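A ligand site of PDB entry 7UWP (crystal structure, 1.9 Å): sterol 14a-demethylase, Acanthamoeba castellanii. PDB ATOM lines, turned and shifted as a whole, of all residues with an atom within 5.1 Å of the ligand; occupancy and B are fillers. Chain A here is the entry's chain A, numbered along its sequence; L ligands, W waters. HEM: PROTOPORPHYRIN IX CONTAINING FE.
SG of Cys 402 is bound to FE of the ligand (2.3 Å). The side-chain hydroxyl (OH) of Tyr 82 lies within hydrogen-bond range of an oxygen (O2A) of the ligand. A ring nitrogen (ND1) of His 400 is in hydrogen-bond range of an oxygen (O1D) of the ligand, 2.6 Å away. An oxygen (O1A) of the ligand is in salt-bridge range of the guanidinium group (NH2) of Arg 336. O2D of the ligand lies within hydrogen-bond range of OH of Tyr 95, 2.9 Å away.
Water W3 lies within hydrogen-bond range of the backbone NH of Met 335 (2.9 Å), an oxygen (O2A) of the ligand (3.3 Å) and the side-chain hydroxyl of Tyr 82 (3.3 Å).
The backbone NH (N) of Gly 404 sits close to the side-chain sulfur (SG) of Cys 402 (3.2 Å). The backbone carbonyl oxygen (O) of Phe 395 lies within hydrogen-bond range of the backbone NH (N) of Cys 402. The side-chain sulfur of Cys 402 lies close to the backbone NH of Glu 405 (3.4 Å). ND1 of His 400 lies close to OE1 of Gln 78 (3.3 Å). O of Ala 262 is in hydrogen-bond range of OG1 of Thr 266 (2.7 Å). The side-chain hydroxyl (OG) of Ser 267 is in hydrogen-bond range of the backbone carbonyl oxygen (O) of Gly 263 (2.7 Å). The backbone carbonyl oxygen (O) of Thr 266 lies within hydrogen-bond range of the side-chain hydroxyl (OG1) of Thr 270, 2.9 Å away.
Merely in contact with the ligand: Gln 78, Leu 106, Leu 113, Ala 262, Gly 263, Thr 266, Ser 267, Thr 270, Leu 325, Pro 330, Val 334, Gly 394, Phe 395, Gly 396, Gly 401, Met 403, Gly 404 and Ala 408. Hydrophobic or aromatic side chains that line the ligand: Tyr 82, Tyr 95, Leu 106, Leu 113, Ala 262, Leu 325, Pro 330, Val 334, Phe 395, His 400, Met 403 and Ala 408. Along chain A the residues within 4 Å of the ligand span positions 78 to 408.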
ATOM      1  N   GLN A  78     -26.697 -16.901   4.803  1.00  0.00           N
ATOM      2  CA  GLN A  78     -25.213 -16.938   4.934  1.00  0.00           C
ATOM      3  C   GLN A  78     -24.792 -17.814   6.122  1.00  0.00           C
ATOM      4  O   GLN A  78     -23.602 -18.059   6.284  1.00  0.00           O
ATOM      5  CB  GLN A  78     -24.654 -15.533   5.149  1.00  0.00           C
ATOM      6  CG  GLN A  78     -24.770 -14.614   3.948  1.00  0.00           C
ATOM      7  CD  GLN A  78     -24.174 -13.268   4.285  1.00  0.00           C
ATOM      8  OE1 GLN A  78     -24.618 -12.587   5.212  1.00  0.00           O
ATOM      9  NE2 GLN A  78     -23.148 -12.888   3.554  1.00  0.00           N
ATOM     10  N   TYR A  82     -20.997 -19.575   6.575  1.00  0.00           N
ATOM     11  CA  TYR A  82     -20.063 -18.760   7.401  1.00  0.00           C
ATOM     12  C   TYR A  82     -19.969 -19.314   8.815  1.00  0.00           C
ATOM     13  O   TYR A  82     -19.349 -18.656   9.657  1.00  0.00           O
ATOM     14  CB  TYR A  82     -20.450 -17.280   7.415  1.00  0.00           C
ATOM     15  CG  TYR A  82     -20.041 -16.540   6.173  1.00  0.00           C
ATOM     16  CD1 TYR A  82     -20.870 -16.500   5.069  1.00  0.00           C
ATOM     17  CD2 TYR A  82     -18.799 -15.930   6.069  1.00  0.00           C
ATOM     18  CE1 TYR A  82     -20.532 -15.786   3.933  1.00  0.00           C
ATOM     19  CE2 TYR A  82     -18.431 -15.239   4.927  1.00  0.00           C
ATOM     20  CZ  TYR A  82     -19.289 -15.178   3.852  1.00  0.00           C
ATOM     21  OH  TYR A  82     -18.938 -14.498   2.719  1.00  0.00           O
ATOM     22  N   TYR A  95     -22.064 -13.489  11.900  1.00  0.00           N
ATOM     23  CA  TYR A  95     -22.758 -14.730  11.468  1.00  0.00           C
ATOM     24  C   TYR A  95     -23.014 -15.622  12.689  1.00  0.00           C
ATOM     25  O   TYR A  95     -23.731 -16.626  12.564  1.00  0.00           O
ATOM     26  CB  TYR A  95     -22.029 -15.422  10.320  1.00  0.00           C
ATOM     27  CG  TYR A  95     -21.637 -14.512   9.191  1.00  0.00           C
ATOM     28  CD1 TYR A  95     -22.578 -13.887   8.386  1.00  0.00           C
ATOM     29  CD2 TYR A  95     -20.303 -14.216   8.953  1.00  0.00           C
ATOM     30  CE1 TYR A  95     -22.204 -13.031   7.360  1.00  0.00           C
ATOM     31  CE2 TYR A  95     -19.922 -13.316   7.982  1.00  0.00           C
ATOM     32  CZ  TYR A  95     -20.865 -12.748   7.148  1.00  0.00           C
ATOM     33  OH  TYR A  95     -20.450 -11.912   6.159  1.00  0.00           O
ATOM     34  N   LEU A 106     -23.815  -4.887  10.979  1.00  0.00           N
ATOM     35  CA  LEU A 106     -23.403  -4.569   9.592  1.00  0.00           C
ATOM     36  C   LEU A 106     -23.574  -3.064   9.340  1.00  0.00           C
ATOM     37  O   LEU A 106     -22.696  -2.484   8.675  1.00  0.00           O
ATOM     38  CB  LEU A 106     -24.215  -5.413   8.598  1.00  0.00           C
ATOM     39  CG  LEU A 106     -23.828  -6.900   8.534  1.00  0.00           C
ATOM     40  CD1 LEU A 106     -24.755  -7.660   7.598  1.00  0.00           C
ATOM     41  CD2 LEU A 106     -22.376  -7.081   8.108  1.00  0.00           C
ATOM     42  N   ILE A 109     -20.536  -1.415  11.005  1.00  0.00           N
ATOM     43  CA  ILE A 109     -19.375  -1.641  10.086  1.00  0.00           C
ATOM     44  C   ILE A 109     -19.478  -0.670   8.907  1.00  0.00           C
ATOM     45  O   ILE A 109     -18.460  -0.026   8.609  1.00  0.00           O
ATOM     46  CB  ILE A 109     -19.287  -3.113   9.631  1.00  0.00           C
ATOM     47  CG1 ILE A 109     -18.872  -4.004  10.800  1.00  0.00           C
ATOM     48  CG2 ILE A 109     -18.358  -3.236   8.439  1.00  0.00           C
ATOM     49  CD1 ILE A 109     -18.863  -5.479  10.510  1.00  0.00           C
ATOM     50  N   LEU A 113     -16.730   2.412   7.750  1.00  0.00           N
ATOM     51  CA  LEU A 113     -16.115   2.340   6.405  1.00  0.00           C
ATOM     52  C   LEU A 113     -16.790   3.321   5.443  1.00  0.00           C
ATOM     53  O   LEU A 113     -16.546   3.224   4.228  1.00  0.00           O
ATOM     54  CB  LEU A 113     -16.217   0.911   5.866  1.00  0.00           C
ATOM     55  CG  LEU A 113     -15.448  -0.137   6.669  1.00  0.00           C
ATOM     56  CD1 LEU A 113     -15.737  -1.526   6.136  1.00  0.00           C
ATOM     57  CD2 LEU A 113     -13.955   0.156   6.656  1.00  0.00           C
ATOM     58  N   LEU A 259     -13.262  -7.776  10.425  1.00  0.00           N
ATOM     59  CA  LEU A 259     -12.707  -6.861   9.387  1.00  0.00           C
ATOM     60  C   LEU A 259     -11.273  -7.272   9.008  1.00  0.00           C
ATOM     61  O   LEU A 259     -10.906  -7.091   7.848  1.00  0.00           O
ATOM     62  CB  LEU A 259     -12.770  -5.421   9.889  1.00  0.00           C
ATOM     63  CG  LEU A 259     -14.177  -4.873  10.090  1.00  0.00           C
ATOM     64  CD1 LEU A 259     -14.113  -3.413  10.493  1.00  0.00           C
ATOM     65  CD2 LEU A 259     -15.020  -5.041   8.838  1.00  0.00           C
ATOM     66  N   ALA A 262     -11.988 -10.157   6.719  1.00  0.00           N
ATOM     67  CA  ALA A 262     -12.583  -9.649   5.455  1.00  0.00           C
ATOM     68  C   ALA A 262     -11.490  -9.009   4.588  1.00  0.00           C
ATOM     69  O   ALA A 262     -11.554  -9.168   3.355  1.00  0.00           O
ATOM     70  CB  ALA A 262     -13.714  -8.690   5.742  1.00  0.00           C
ATOM     71  N   GLY A 263     -10.526  -8.321   5.217  1.00  0.00           N
ATOM     72  CA  GLY A 263      -9.800  -7.194   4.601  1.00  0.00           C
ATOM     73  C   GLY A 263      -8.318  -7.459   4.377  1.00  0.00           C
ATOM     74  O   GLY A 263      -7.721  -6.716   3.574  1.00  0.00           O
ATOM     75  N   THR A 266      -7.396 -10.684   1.298  1.00  0.00           N
ATOM     76  CA  THR A 266      -8.068 -10.197   0.063  1.00  0.00           C
ATOM     77  C   THR A 266      -7.287  -9.008  -0.500  1.00  0.00           C
ATOM     78  O   THR A 266      -7.018  -9.001  -1.713  1.00  0.00           O
ATOM     79  CB  THR A 266      -9.536  -9.822   0.317  1.00  0.00           C
ATOM     80  OG1 THR A 266      -9.592  -9.037   1.505  1.00  0.00           O
ATOM     81  CG2 THR A 266     -10.404 -11.049   0.458  1.00  0.00           C
ATOM     82  N   SER A 267      -7.004  -7.998   0.324  1.00  0.00           N
ATOM     83  CA  SER A 267      -6.394  -6.715  -0.130  1.00  0.00           C
ATOM     84  C   SER A 267      -4.925  -6.964  -0.514  1.00  0.00           C
ATOM     85  O   SER A 267      -4.494  -6.487  -1.562  1.00  0.00           O
ATOM     86  CB  SER A 267      -6.509  -5.645   0.930  1.00  0.00           C
ATOM     87  OG  SER A 267      -7.859  -5.377   1.251  1.00  0.00           O
ATOM     88  N   THR A 270      -4.745  -8.988  -3.856  1.00  0.00           N
ATOM     89  CA  THR A 270      -5.176  -8.072  -4.952  1.00  0.00           C
ATOM     90  C   THR A 270      -4.105  -6.996  -5.170  1.00  0.00           C
ATOM     91  O   THR A 270      -3.737  -6.762  -6.338  1.00  0.00           O
ATOM     92  CB  THR A 270      -6.572  -7.493  -4.715  1.00  0.00           C
ATOM     93  OG1 THR A 270      -7.476  -8.599  -4.573  1.00  0.00           O
ATOM     94  CG2 THR A 270      -7.023  -6.588  -5.846  1.00  0.00           C
ATOM     95  N   LEU A 325      -8.127  -7.968 -10.087  1.00  0.00           N
ATOM     96  CA  LEU A 325      -9.255  -8.554  -9.334  1.00  0.00           C
ATOM     97  C   LEU A 325     -10.139  -9.374 -10.288  1.00  0.00           C
ATOM     98  O   LEU A 325     -10.491 -10.531  -9.934  1.00  0.00           O
ATOM     99  CB  LEU A 325     -10.024  -7.435  -8.648  1.00  0.00           C
ATOM    100  CG  LEU A 325     -11.231  -7.891  -7.834  1.00  0.00           C
ATOM    101  CD1 LEU A 325     -10.814  -8.947  -6.817  1.00  0.00           C
ATOM    102  CD2 LEU A 325     -11.899  -6.700  -7.147  1.00  0.00           C
ATOM    103  N   PRO A 330      -9.690 -13.056  -5.150  1.00  0.00           N
ATOM    104  CA  PRO A 330      -9.200 -13.777  -3.979  1.00  0.00           C
ATOM    105  C   PRO A 330     -10.198 -14.781  -3.365  1.00  0.00           C
ATOM    106  O   PRO A 330      -9.767 -15.714  -2.734  1.00  0.00           O
ATOM    107  CB  PRO A 330      -8.855 -12.659  -2.990  1.00  0.00           C
ATOM    108  CG  PRO A 330      -9.720 -11.487  -3.422  1.00  0.00           C
ATOM    109  CD  PRO A 330      -9.860 -11.615  -4.919  1.00  0.00           C
ATOM    110  N   LEU A 331     -11.497 -14.558  -3.536  1.00  0.00           N
ATOM    111  CA  LEU A 331     -12.531 -15.544  -3.120  1.00  0.00           C
ATOM    112  C   LEU A 331     -13.143 -16.181  -4.365  1.00  0.00           C
ATOM    113  O   LEU A 331     -13.687 -15.449  -5.197  1.00  0.00           O
ATOM    114  CB  LEU A 331     -13.573 -14.817  -2.261  1.00  0.00           C
ATOM    115  CG  LEU A 331     -12.979 -14.162  -1.015  1.00  0.00           C
ATOM    116  CD1 LEU A 331     -13.938 -13.169  -0.394  1.00  0.00           C
ATOM    117  CD2 LEU A 331     -12.558 -15.226  -0.002  1.00  0.00           C
ATOM    118  N   VAL A 334     -18.680 -17.420  -3.669  1.00  0.00           N
ATOM    119  CA  VAL A 334     -19.640 -16.973  -2.615  1.00  0.00           C
ATOM    120  C   VAL A 334     -20.844 -17.900  -2.669  1.00  0.00           C
ATOM    121  O   VAL A 334     -21.124 -18.488  -3.737  1.00  0.00           O
ATOM    122  CB  VAL A 334     -20.035 -15.492  -2.794  1.00  0.00           C
ATOM    123  CG1 VAL A 334     -18.844 -14.568  -2.555  1.00  0.00           C
ATOM    124  CG2 VAL A 334     -20.659 -15.230  -4.153  1.00  0.00           C
ATOM    125  N   MET A 335     -21.429 -18.182  -1.510  1.00  0.00           N
ATOM    126  CA  MET A 335     -22.427 -19.268  -1.417  1.00  0.00           C
ATOM    127  C   MET A 335     -23.490 -18.949  -0.370  1.00  0.00           C
ATOM    128  O   MET A 335     -23.270 -18.104   0.533  1.00  0.00           O
ATOM    129  CB  MET A 335     -21.758 -20.617  -1.132  1.00  0.00           C
ATOM    130  CG  MET A 335     -21.183 -20.746   0.260  1.00  0.00           C
ATOM    131  SD  MET A 335     -20.192 -22.269   0.498  1.00  0.00           S
ATOM    132  CE  MET A 335     -18.703 -21.804  -0.389  1.00  0.00           C
ATOM    133  N   ARG A 336     -24.660 -19.527  -0.586  1.00  0.00           N
ATOM    134  CA  ARG A 336     -25.859 -19.293   0.255  1.00  0.00           C
ATOM    135  C   ARG A 336     -26.556 -20.636   0.388  1.00  0.00           C
ATOM    136  O   ARG A 336     -26.621 -21.391  -0.596  1.00  0.00           O
ATOM    137  CB  ARG A 336     -26.789 -18.256  -0.379  1.00  0.00           C
ATOM    138  CG  ARG A 336     -26.153 -16.909  -0.658  1.00  0.00           C
ATOM    139  CD  ARG A 336     -25.929 -16.094   0.607  1.00  0.00           C
ATOM    140  NE  ARG A 336     -25.523 -14.740   0.260  1.00  0.00           N
ATOM    141  CZ  ARG A 336     -24.265 -14.312   0.186  1.00  0.00           C
ATOM    142  NH1 ARG A 336     -23.267 -15.141   0.463  1.00  0.00           N
ATOM    143  NH2 ARG A 336     -24.007 -13.079  -0.211  1.00  0.00           N
ATOM    144  N   VAL A 393     -18.195  -9.012 -10.410  1.00  0.00           N
ATOM    145  CA  VAL A 393     -18.659  -9.513  -9.092  1.00  0.00           C
ATOM    146  C   VAL A 393     -17.440  -9.903  -8.231  1.00  0.00           C
ATOM    147  O   VAL A 393     -17.609 -10.720  -7.313  1.00  0.00           O
ATOM    148  CB  VAL A 393     -19.630 -10.702  -9.263  1.00  0.00           C
ATOM    149  CG1 VAL A 393     -20.931 -10.271  -9.934  1.00  0.00           C
ATOM    150  CG2 VAL A 393     -18.980 -11.828 -10.051  1.00  0.00           C
ATOM    151  N   GLY A 394     -16.299  -9.268  -8.460  1.00  0.00           N
ATOM    152  CA  GLY A 394     -15.093  -9.427  -7.628  1.00  0.00           C
ATOM    153  C   GLY A 394     -15.369  -9.108  -6.168  1.00  0.00           C
ATOM    154  O   GLY A 394     -14.797  -9.798  -5.310  1.00  0.00           O
ATOM    155  N   PHE A 395     -16.228  -8.133  -5.889  1.00  0.00           N
ATOM    156  CA  PHE A 395     -16.588  -7.685  -4.515  1.00  0.00           C
ATOM    157  C   PHE A 395     -18.002  -8.180  -4.153  1.00  0.00           C
ATOM    158  O   PHE A 395     -18.668  -7.595  -3.258  1.00  0.00           O
ATOM    159  CB  PHE A 395     -16.537  -6.162  -4.375  1.00  0.00           C
ATOM    160  CG  PHE A 395     -15.162  -5.561  -4.445  1.00  0.00           C
ATOM    161  CD1 PHE A 395     -14.334  -5.540  -3.321  1.00  0.00           C
ATOM    162  CD2 PHE A 395     -14.677  -5.015  -5.620  1.00  0.00           C
ATOM    163  CE1 PHE A 395     -13.079  -4.961  -3.387  1.00  0.00           C
ATOM    164  CE2 PHE A 395     -13.412  -4.461  -5.677  1.00  0.00           C
ATOM    165  CZ  PHE A 395     -12.622  -4.425  -4.560  1.00  0.00           C
ATOM    166  N   GLY A 396     -18.453  -9.237  -4.813  1.00  0.00           N
ATOM    167  CA  GLY A 396     -19.865  -9.652  -4.708  1.00  0.00           C
ATOM    168  C   GLY A 396     -20.792  -8.549  -5.184  1.00  0.00           C
ATOM    169  O   GLY A 396     -20.371  -7.741  -6.039  1.00  0.00           O
ATOM    170  N   ARG A 399     -27.206  -7.221  -1.420  1.00  0.00           N
ATOM    171  CA  ARG A 399     -27.319  -6.883   0.024  1.00  0.00           C
ATOM    172  C   ARG A 399     -25.965  -7.049   0.749  1.00  0.00           C
ATOM    173  O   ARG A 399     -25.670  -6.233   1.643  1.00  0.00           O
ATOM    174  CB  ARG A 399     -28.365  -7.787   0.643  1.00  0.00           C
ATOM    175  CG  ARG A 399     -28.406  -7.660   2.158  1.00  0.00           C
ATOM    176  CD  ARG A 399     -28.909  -6.284   2.547  1.00  0.00           C
ATOM    177  NE  ARG A 399     -28.515  -5.964   3.911  1.00  0.00           N
ATOM    178  CZ  ARG A 399     -28.955  -6.584   4.991  1.00  0.00           C
ATOM    179  NH1 ARG A 399     -29.872  -7.536   4.905  1.00  0.00           N
ATOM    180  NH2 ARG A 399     -28.469  -6.245   6.172  1.00  0.00           N
ATOM    181  N   HIS A 400     -25.265  -8.163   0.528  1.00  0.00           N
ATOM    182  CA  HIS A 400     -24.011  -8.490   1.263  1.00  0.00           C
ATOM    183  C   HIS A 400     -22.765  -8.224   0.424  1.00  0.00           C
ATOM    184  O   HIS A 400     -21.701  -8.768   0.773  1.00  0.00           O
ATOM    185  CB  HIS A 400     -24.079  -9.926   1.788  1.00  0.00           C
ATOM    186  CG  HIS A 400     -25.120 -10.091   2.826  1.00  0.00           C
ATOM    187  ND1 HIS A 400     -25.003  -9.530   4.089  1.00  0.00           N
ATOM    188  CD2 HIS A 400     -26.365 -10.623   2.775  1.00  0.00           C
ATOM    189  CE1 HIS A 400     -26.082  -9.799   4.785  1.00  0.00           C
ATOM    190  NE2 HIS A 400     -26.941 -10.469   4.004  1.00  0.00           N
ATOM    191  N   GLY A 401     -22.870  -7.343  -0.582  1.00  0.00           N
ATOM    192  CA  GLY A 401     -21.723  -6.806  -1.342  1.00  0.00           C
ATOM    193  C   GLY A 401     -20.662  -6.259  -0.395  1.00  0.00           C
ATOM    194  O   GLY A 401     -21.009  -5.789   0.701  1.00  0.00           O
ATOM    195  N   CYS A 402     -19.385  -6.341  -0.788  1.00  0.00           N
ATOM    196  CA  CYS A 402     -18.256  -5.869   0.059  1.00  0.00           C
ATOM    197  C   CYS A 402     -18.474  -4.419   0.534  1.00  0.00           C
ATOM    198  O   CYS A 402     -18.521  -3.504  -0.308  1.00  0.00           O
ATOM    199  CB  CYS A 402     -16.934  -5.965  -0.694  1.00  0.00           C
ATOM    200  SG  CYS A 402     -15.510  -5.549   0.343  1.00  0.00           S
ATOM    201  N   MET A 403     -18.419  -4.199   1.845  1.00  0.00           N
ATOM    202  CA  MET A 403     -18.469  -2.840   2.453  1.00  0.00           C
ATOM    203  C   MET A 403     -17.058  -2.233   2.537  1.00  0.00           C
ATOM    204  O   MET A 403     -16.955  -1.005   2.779  1.00  0.00           O
ATOM    205  CB  MET A 403     -19.068  -2.917   3.856  1.00  0.00           C
ATOM    206  CG  MET A 403     -20.528  -3.327   3.859  1.00  0.00           C
ATOM    207  SD  MET A 403     -21.305  -2.969   5.466  1.00  0.00           S
ATOM    208  CE  MET A 403     -20.856  -4.430   6.386  1.00  0.00           C
ATOM    209  N   GLY A 404     -16.010  -3.023   2.285  1.00  0.00           N
ATOM    210  CA  GLY A 404     -14.621  -2.536   2.313  1.00  0.00           C
ATOM    211  C   GLY A 404     -14.097  -2.111   0.955  1.00  0.00           C
ATOM    212  O   GLY A 404     -12.907  -1.761   0.868  1.00  0.00           O
ATOM    213  N   GLU A 405     -14.925  -2.212  -0.095  1.00  0.00           N
ATOM    214  CA  GLU A 405     -14.465  -2.019  -1.488  1.00  0.00           C
ATOM    215  C   GLU A 405     -13.684  -0.695  -1.559  1.00  0.00           C
ATOM    216  O   GLU A 405     -12.567  -0.706  -2.086  1.00  0.00           O
ATOM    217  CB  GLU A 405     -15.641  -2.010  -2.460  1.00  0.00           C
ATOM    218  CG  GLU A 405     -15.225  -1.704  -3.888  1.00  0.00           C
ATOM    219  CD  GLU A 405     -16.336  -1.874  -4.907  1.00  0.00           C
ATOM    220  OE1 GLU A 405     -17.358  -2.499  -4.541  1.00  0.00           O
ATOM    221  OE2 GLU A 405     -16.148  -1.473  -6.075  1.00  0.00           O
ATOM    222  N   PHE A 407     -12.368   1.360   0.709  1.00  0.00           N
ATOM    223  CA  PHE A 407     -11.135   1.241   1.531  1.00  0.00           C
ATOM    224  C   PHE A 407     -10.057   0.431   0.793  1.00  0.00           C
ATOM    225  O   PHE A 407      -8.877   0.845   0.799  1.00  0.00           O
ATOM    226  CB  PHE A 407     -11.465   0.612   2.879  1.00  0.00           C
ATOM    227  CG  PHE A 407     -10.286   0.562   3.818  1.00  0.00           C
ATOM    228  CD1 PHE A 407      -9.298  -0.395   3.690  1.00  0.00           C
ATOM    229  CD2 PHE A 407     -10.162   1.505   4.827  1.00  0.00           C
ATOM    230  CE1 PHE A 407      -8.210  -0.412   4.540  1.00  0.00           C
ATOM    231  CE2 PHE A 407      -9.086   1.467   5.704  1.00  0.00           C
ATOM    232  CZ  PHE A 407      -8.105   0.523   5.549  1.00  0.00           C
ATOM    233  N   ALA A 408     -10.421  -0.733   0.243  1.00  0.00           N
ATOM    234  CA  ALA A 408      -9.487  -1.616  -0.499  1.00  0.00           C
ATOM    235  C   ALA A 408      -8.831  -0.839  -1.653  1.00  0.00           C
ATOM    236  O   ALA A 408      -7.598  -0.923  -1.820  1.00  0.00           O
ATOM    237  CB  ALA A 408     -10.211  -2.840  -0.997  1.00  0.00           C
ATOM    238  N   ILE A 412      -4.807   0.083  -1.978  1.00  0.00           N
ATOM    239  CA  ILE A 412      -3.983  -0.515  -3.065  1.00  0.00           C
ATOM    240  C   ILE A 412      -3.477   0.597  -3.992  1.00  0.00           C
ATOM    241  O   ILE A 412      -2.329   0.513  -4.437  1.00  0.00           O
ATOM    242  CB  ILE A 412      -4.788  -1.606  -3.797  1.00  0.00           C
ATOM    243  CG1 ILE A 412      -5.058  -2.774  -2.838  1.00  0.00           C
ATOM    244  CG2 ILE A 412      -4.077  -2.066  -5.063  1.00  0.00           C
ATOM    245  CD1 ILE A 412      -6.112  -3.745  -3.326  1.00  0.00           C
HETATM  246  CHA HEM L   1     -17.952  -8.899   1.810  1.00  0.00           C
HETATM  247  CHB HEM L   1     -14.494  -9.291  -1.531  1.00  0.00           C
HETATM  248  CHC HEM L   1     -11.691  -6.163   0.983  1.00  0.00           C
HETATM  249  CHD HEM L   1     -15.110  -5.951   4.406  1.00  0.00           C
HETATM  250  C1A HEM L   1     -17.237  -9.240   0.694  1.00  0.00           C
HETATM  251  C2A HEM L   1     -17.699 -10.163  -0.283  1.00  0.00           C
HETATM  252  C3A HEM L   1     -16.716 -10.287  -1.214  1.00  0.00           C
HETATM  253  C4A HEM L   1     -15.658  -9.449  -0.828  1.00  0.00           C
HETATM  254  CMA HEM L   1     -16.781 -11.125  -2.469  1.00  0.00           C
HETATM  255  CAA HEM L   1     -19.071 -10.838  -0.331  1.00  0.00           C
HETATM  256  CBA HEM L   1     -19.135 -12.075   0.580  1.00  0.00           C
HETATM  257  CGA HEM L   1     -20.462 -12.800   0.416  1.00  0.00           C
HETATM  258  O1A HEM L   1     -21.291 -12.454  -0.465  1.00  0.00           O
HETATM  259  O2A HEM L   1     -20.732 -13.762   1.170  1.00  0.00           O
HETATM  260  C1B HEM L   1     -13.444  -8.457  -1.100  1.00  0.00           C
HETATM  261  C2B HEM L   1     -12.270  -8.249  -1.884  1.00  0.00           C
HETATM  262  C3B HEM L   1     -11.477  -7.385  -1.184  1.00  0.00           C
HETATM  263  C4B HEM L   1     -12.222  -7.041   0.032  1.00  0.00           C
HETATM  264  CMB HEM L   1     -11.944  -8.888  -3.220  1.00  0.00           C
HETATM  265  CAB HEM L   1     -10.140  -6.794  -1.468  1.00  0.00           C
HETATM  266  CBB HEM L   1      -9.722  -6.472  -2.694  1.00  0.00           C
HETATM  267  C1C HEM L   1     -12.358  -5.858   2.148  1.00  0.00           C
HETATM  268  C2C HEM L   1     -11.904  -5.002   3.152  1.00  0.00           C
HETATM  269  C3C HEM L   1     -12.887  -4.956   4.134  1.00  0.00           C
HETATM  270  C4C HEM L   1     -13.945  -5.798   3.712  1.00  0.00           C
HETATM  271  CMC HEM L   1     -10.580  -4.260   3.118  1.00  0.00           C
HETATM  272  CAC HEM L   1     -12.885  -4.229   5.416  1.00  0.00           C
HETATM  273  CBC HEM L   1     -12.062  -3.238   5.670  1.00  0.00           C
HETATM  274  C1D HEM L   1     -16.104  -6.771   3.924  1.00  0.00           C
HETATM  275  C2D HEM L   1     -17.346  -6.916   4.663  1.00  0.00           C
HETATM  276  C3D HEM L   1     -18.119  -7.745   3.976  1.00  0.00           C
HETATM  277  C4D HEM L   1     -17.397  -8.034   2.736  1.00  0.00           C
HETATM  278  CMD HEM L   1     -17.693  -6.362   6.007  1.00  0.00           C
HETATM  279  CAD HEM L   1     -19.434  -8.315   4.506  1.00  0.00           C
HETATM  280  CBD HEM L   1     -20.670  -7.834   3.810  1.00  0.00           C
HETATM  281  CGD HEM L   1     -21.867  -8.596   4.387  1.00  0.00           C
HETATM  282  O1D HEM L   1     -22.915  -7.969   4.443  1.00  0.00           O
HETATM  283  O2D HEM L   1     -21.872  -9.816   4.790  1.00  0.00           O
HETATM  284  NA  HEM L   1     -15.953  -8.849   0.390  1.00  0.00           N
HETATM  285  NB  HEM L   1     -13.374  -7.702   0.009  1.00  0.00           N
HETATM  286  NC  HEM L   1     -13.624  -6.267   2.474  1.00  0.00           N
HETATM  287  ND  HEM L   1     -16.172  -7.451   2.749  1.00  0.00           N
HETATM  288 FE   HEM L   1     -14.883  -7.470   1.390  1.00  0.00          FE
HETATM  289  O   HOH W   1     -14.011  -9.662   2.242  1.00  0.00           O
HETATM  290  O   HOH W   2     -22.109 -10.504  -2.276  1.00  0.00           O
HETATM  291  O   HOH W   3     -19.955 -16.874   0.619  1.00  0.00           O
HETATM  292  O   HOH W   4     -15.909 -11.757   2.685  1.00  0.00           O
